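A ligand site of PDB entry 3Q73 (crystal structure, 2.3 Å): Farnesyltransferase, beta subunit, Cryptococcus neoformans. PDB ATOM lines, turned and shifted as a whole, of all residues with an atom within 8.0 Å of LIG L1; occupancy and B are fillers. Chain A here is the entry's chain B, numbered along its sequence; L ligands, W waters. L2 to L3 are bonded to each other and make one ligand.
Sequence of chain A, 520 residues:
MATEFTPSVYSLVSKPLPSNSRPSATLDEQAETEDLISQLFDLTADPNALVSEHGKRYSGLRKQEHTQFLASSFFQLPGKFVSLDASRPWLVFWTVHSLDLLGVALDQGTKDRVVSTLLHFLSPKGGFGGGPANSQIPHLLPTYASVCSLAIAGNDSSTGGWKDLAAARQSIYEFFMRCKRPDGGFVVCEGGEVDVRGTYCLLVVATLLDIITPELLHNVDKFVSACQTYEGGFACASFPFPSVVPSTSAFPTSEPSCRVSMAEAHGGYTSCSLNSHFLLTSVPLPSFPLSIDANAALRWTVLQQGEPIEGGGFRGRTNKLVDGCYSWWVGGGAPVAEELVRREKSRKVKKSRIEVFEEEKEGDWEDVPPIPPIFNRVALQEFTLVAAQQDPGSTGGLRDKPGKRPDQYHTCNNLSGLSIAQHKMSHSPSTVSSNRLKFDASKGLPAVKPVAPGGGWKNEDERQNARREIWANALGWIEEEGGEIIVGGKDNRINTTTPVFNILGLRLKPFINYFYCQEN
Water W1 lies within hydrogen-bond range of O4 of LIG L1 (2.8 Å) and O1 of LG2 L2 (2.8 Å).
Water W2 lies within hydrogen-bond range of N1 of LIG L1 (2.9 Å), O of Gly 488 (2.9 Å) and N of Asp 491 (3.4 Å).
N of Asp 491 is in hydrogen-bond range of O3 of LIG L1, at 3.4 Å.
The side-chain carboxylate (OD2) of Asp 491 lies within salt-bridge range of a nitrogen (N1) of LIG L1 (2.6 Å).
N of Lys 490 is in hydrogen-bond range of O4 of LIG L1 (2.9 Å).
O3 of LG2 L2 lies within hydrogen-bond range of N of Gly 488 (2.8 Å).
The backbone NH of Ile 486 lies within hydrogen-bond range of an oxygen (O4) of LG3 L3, 2.7 Å away.
An oxygen (O3) of LG3 L3 sits at hydrogen-bond distance from the backbone carbonyl oxygen of Ile 486.
Residues that only touch LIG L1: Gly 489 (3.3 Å) and Tyr 58 (3.4 Å).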
ATOM      1  N   TYR A  58     -37.803  20.635  25.390  1.00  0.00           N
ATOM      2  CA  TYR A  58     -36.520  21.211  25.007  1.00  0.00           C
ATOM      3  C   TYR A  58     -36.753  22.484  24.176  1.00  0.00           C
ATOM      4  O   TYR A  58     -37.605  22.508  23.282  1.00  0.00           O
ATOM      5  CB  TYR A  58     -35.640  20.190  24.268  1.00  0.00           C
ATOM      6  CG  TYR A  58     -34.306  20.774  23.826  1.00  0.00           C
ATOM      7  CD1 TYR A  58     -33.957  20.809  22.482  1.00  0.00           C
ATOM      8  CD2 TYR A  58     -33.428  21.325  24.770  1.00  0.00           C
ATOM      9  CE1 TYR A  58     -32.738  21.365  22.068  1.00  0.00           C
ATOM     10  CE2 TYR A  58     -32.214  21.876  24.368  1.00  0.00           C
ATOM     11  CZ  TYR A  58     -31.882  21.898  23.021  1.00  0.00           C
ATOM     12  OH  TYR A  58     -30.678  22.452  22.633  1.00  0.00           O
ATOM     13  N   GLY A  60     -34.529  24.270  22.297  1.00  0.00           N
ATOM     14  CA  GLY A  60     -33.609  24.535  21.181  1.00  0.00           C
ATOM     15  C   GLY A  60     -34.297  25.148  19.978  1.00  0.00           C
ATOM     16  O   GLY A  60     -35.450  24.839  19.695  1.00  0.00           O
ATOM     17  N   LEU A  61     -33.590  26.033  19.273  1.00  0.00           N
ATOM     18  CA  LEU A  61     -34.121  26.629  18.056  1.00  0.00           C
ATOM     19  C   LEU A  61     -34.312  25.544  16.998  1.00  0.00           C
ATOM     20  O   LEU A  61     -33.358  24.862  16.613  1.00  0.00           O
ATOM     21  CB  LEU A  61     -33.203  27.749  17.540  1.00  0.00           C
ATOM     22  CG  LEU A  61     -33.753  28.627  16.406  1.00  0.00           C
ATOM     23  CD1 LEU A  61     -35.028  29.336  16.822  1.00  0.00           C
ATOM     24  CD2 LEU A  61     -32.714  29.641  15.973  1.00  0.00           C
ATOM     25  N   ILE A 486     -25.148  33.637  23.206  1.00  0.00           N
ATOM     26  CA  ILE A 486     -26.075  32.685  22.596  1.00  0.00           C
ATOM     27  C   ILE A 486     -26.707  31.796  23.668  1.00  0.00           C
ATOM     28  O   ILE A 486     -26.137  30.776  24.078  1.00  0.00           O
ATOM     29  CB  ILE A 486     -25.404  31.816  21.489  1.00  0.00           C
ATOM     30  CG1 ILE A 486     -24.481  32.658  20.598  1.00  0.00           C
ATOM     31  CG2 ILE A 486     -26.476  31.075  20.683  1.00  0.00           C
ATOM     32  CD1 ILE A 486     -25.183  33.686  19.722  1.00  0.00           C
ATOM     33  N   VAL A 487     -27.898  32.199  24.111  1.00  0.00           N
ATOM     34  CA  VAL A 487     -28.635  31.487  25.149  1.00  0.00           C
ATOM     35  C   VAL A 487     -28.959  30.076  24.661  1.00  0.00           C
ATOM     36  O   VAL A 487     -29.476  29.898  23.556  1.00  0.00           O
ATOM     37  CB  VAL A 487     -29.913  32.258  25.547  1.00  0.00           C
ATOM     38  CG1 VAL A 487     -30.817  31.427  26.472  1.00  0.00           C
ATOM     39  CG2 VAL A 487     -29.554  33.591  26.193  1.00  0.00           C
ATOM     40  N   GLY A 488     -28.613  29.084  25.471  1.00  0.00           N
ATOM     41  CA  GLY A 488     -28.905  27.680  25.173  1.00  0.00           C
ATOM     42  C   GLY A 488     -27.837  26.950  24.380  1.00  0.00           C
ATOM     43  O   GLY A 488     -28.005  25.773  24.044  1.00  0.00           O
ATOM     44  N   GLY A 489     -26.748  27.635  24.071  1.00  0.00           N
ATOM     45  CA  GLY A 489     -25.636  27.007  23.356  1.00  0.00           C
ATOM     46  C   GLY A 489     -25.530  27.436  21.906  1.00  0.00           C
ATOM     47  O   GLY A 489     -26.464  28.034  21.359  1.00  0.00           O
ATOM     48  N   LYS A 490     -24.403  27.102  21.283  1.00  0.00           N
ATOM     49  CA  LYS A 490     -24.081  27.647  19.962  1.00  0.00           C
ATOM     50  C   LYS A 490     -24.927  27.103  18.818  1.00  0.00           C
ATOM     51  O   LYS A 490     -24.978  27.702  17.750  1.00  0.00           O
ATOM     52  CB  LYS A 490     -22.585  27.492  19.667  1.00  0.00           C
ATOM     53  CG  LYS A 490     -21.713  28.360  20.569  1.00  0.00           C
ATOM     54  CD  LYS A 490     -20.243  28.198  20.261  1.00  0.00           C
ATOM     55  CE  LYS A 490     -19.427  29.256  20.976  1.00  0.00           C
ATOM     56  NZ  LYS A 490     -17.965  29.166  20.660  1.00  0.00           N
ATOM     57  N   ASP A 491     -25.619  25.986  19.033  1.00  0.00           N
ATOM     58  CA  ASP A 491     -26.560  25.481  18.028  1.00  0.00           C
ATOM     59  C   ASP A 491     -27.783  26.390  17.853  1.00  0.00           C
ATOM     60  O   ASP A 491     -28.478  26.280  16.846  1.00  0.00           O
ATOM     61  CB  ASP A 491     -26.993  24.047  18.345  1.00  0.00           C
ATOM     62  CG  ASP A 491     -25.904  23.040  18.069  1.00  0.00           C
ATOM     63  OD1 ASP A 491     -25.152  23.189  17.072  1.00  0.00           O
ATOM     64  OD2 ASP A 491     -25.798  22.080  18.853  1.00  0.00           O
ATOM     65  N   ASN A 492     -28.040  27.263  18.823  1.00  0.00           N
ATOM     66  CA  ASN A 492     -29.108  28.261  18.705  1.00  0.00           C
ATOM     67  C   ASN A 492     -28.708  29.502  17.897  1.00  0.00           C
ATOM     68  O   ASN A 492     -29.565  30.309  17.519  1.00  0.00           O
ATOM     69  CB  ASN A 492     -29.631  28.672  20.082  1.00  0.00           C
ATOM     70  CG  ASN A 492     -30.412  27.567  20.766  1.00  0.00           C
ATOM     71  OD1 ASN A 492     -30.907  26.636  20.126  1.00  0.00           O
ATOM     72  ND2 ASN A 492     -30.534  27.672  22.084  1.00  0.00           N
ATOM     73  N   ARG A 493     -27.414  29.644  17.633  1.00  0.00           N
ATOM     74  CA  ARG A 493     -26.895  30.828  16.933  1.00  0.00           C
ATOM     75  C   ARG A 493     -27.523  31.020  15.570  1.00  0.00           C
ATOM     76  O   ARG A 493     -27.604  30.083  14.774  1.00  0.00           O
ATOM     77  CB  ARG A 493     -25.369  30.782  16.793  1.00  0.00           C
ATOM     78  CG  ARG A 493     -24.799  32.028  16.112  1.00  0.00           C
ATOM     79  CD  ARG A 493     -23.344  31.841  15.686  1.00  0.00           C
ATOM     80  NE  ARG A 493     -22.798  33.092  15.149  1.00  0.00           N
ATOM     81  CZ  ARG A 493     -22.937  33.502  13.891  1.00  0.00           C
ATOM     82  NH1 ARG A 493     -23.615  32.771  13.006  1.00  0.00           N
ATOM     83  NH2 ARG A 493     -22.412  34.658  13.510  1.00  0.00           N
HETATM   84  O1  LIG L   1     -20.654  24.495  23.676  1.00  0.00           O
HETATM   85  O2  LIG L   1     -21.354  24.773  21.394  1.00  0.00           O
HETATM   86  O3  LIG L   1     -24.038  23.612  20.913  1.00  0.00           O
HETATM   87  O4  LIG L   1     -22.629  25.754  23.164  1.00  0.00           O
HETATM   88  C1  LIG L   1     -28.409  18.341  20.758  1.00  0.00           C
HETATM   89  C2  LIG L   1     -27.026  18.155  21.302  1.00  0.00           C
HETATM   90  C3  LIG L   1     -29.064  19.585  21.271  1.00  0.00           C
HETATM   91  C4  LIG L   1     -26.186  19.380  21.164  1.00  0.00           C
HETATM   92  C5  LIG L   1     -28.212  20.786  21.080  1.00  0.00           C
HETATM   93  C6  LIG L   1     -25.056  22.043  22.364  1.00  0.00           C
HETATM   94  C7  LIG L   1     -22.801  23.147  22.878  1.00  0.00           C
HETATM   95  N1  LIG L   1     -26.101  21.822  21.405  1.00  0.00           N
HETATM   96  C8  LIG L   1     -23.990  23.023  21.991  1.00  0.00           C
HETATM   97  C9  LIG L   1     -26.869  20.614  21.687  1.00  0.00           C
HETATM   98  S1  LIG L   1     -21.807  24.602  22.778  1.00  0.00           S
HETATM   99  C1  LG2 L   2     -23.358  29.535  27.642  1.00  0.00           C
HETATM  100  C2  LG2 L   2     -24.243  28.359  27.966  1.00  0.00           C
HETATM  101  C3  LG2 L   2     -25.598  28.580  28.568  1.00  0.00           C
HETATM  102  C4  LG2 L   2     -26.192  29.941  28.509  1.00  0.00           C
HETATM  103  C5  LG2 L   2     -25.255  30.880  27.780  1.00  0.00           C
HETATM  104  C6  LG2 L   2     -25.627  32.288  28.089  1.00  0.00           C
HETATM  105  O1  LG2 L   2     -23.766  27.086  27.753  1.00  0.00           O
HETATM  106  O2  LG2 L   2     -26.318  27.493  29.040  1.00  0.00           O
HETATM  107  O3  LG2 L   2     -27.439  29.923  27.888  1.00  0.00           O
HETATM  108  O4  LG2 L   2     -23.893  30.749  28.122  1.00  0.00           O
HETATM  109  O5  LG2 L   2     -25.314  32.618  29.393  1.00  0.00           O
HETATM  110  C1  LG3 L   3     -21.188  28.607  25.551  1.00  0.00           C
HETATM  111  C2  LG3 L   3     -22.011  29.847  25.683  1.00  0.00           C
HETATM  112  C3  LG3 L   3     -22.393  30.442  24.368  1.00  0.00           C
HETATM  113  C4  LG3 L   3     -22.131  31.899  24.405  1.00  0.00           C
HETATM  114  C5  LG3 L   3     -21.587  32.111  25.771  1.00  0.00           C
HETATM  115  C6  LG3 L   3     -21.160  33.440  26.345  1.00  0.00           C
HETATM  116  O1  LG3 L   3     -20.001  28.882  24.900  1.00  0.00           O
HETATM  117  O2  LG3 L   3     -23.259  29.507  26.256  1.00  0.00           O
HETATM  118  O3  LG3 L   3     -23.099  29.805  23.342  1.00  0.00           O
HETATM  119  O4  LG3 L   3     -22.552  32.753  23.373  1.00  0.00           O
HETATM  120  O5  LG3 L   3     -21.320  30.859  26.400  1.00  0.00           O
HETATM  121  O6  LG3 L   3     -21.794  33.563  27.575  1.00  0.00           O
HETATM  122  O   HOH W   1     -23.875  25.347  25.601  1.00  0.00           O
HETATM  123  O   HOH W   2     -27.216  24.469  21.580  1.00  0.00           O
HETATM  124  O   HOH W   3     -30.461  22.169  18.843  1.00  0.00           O
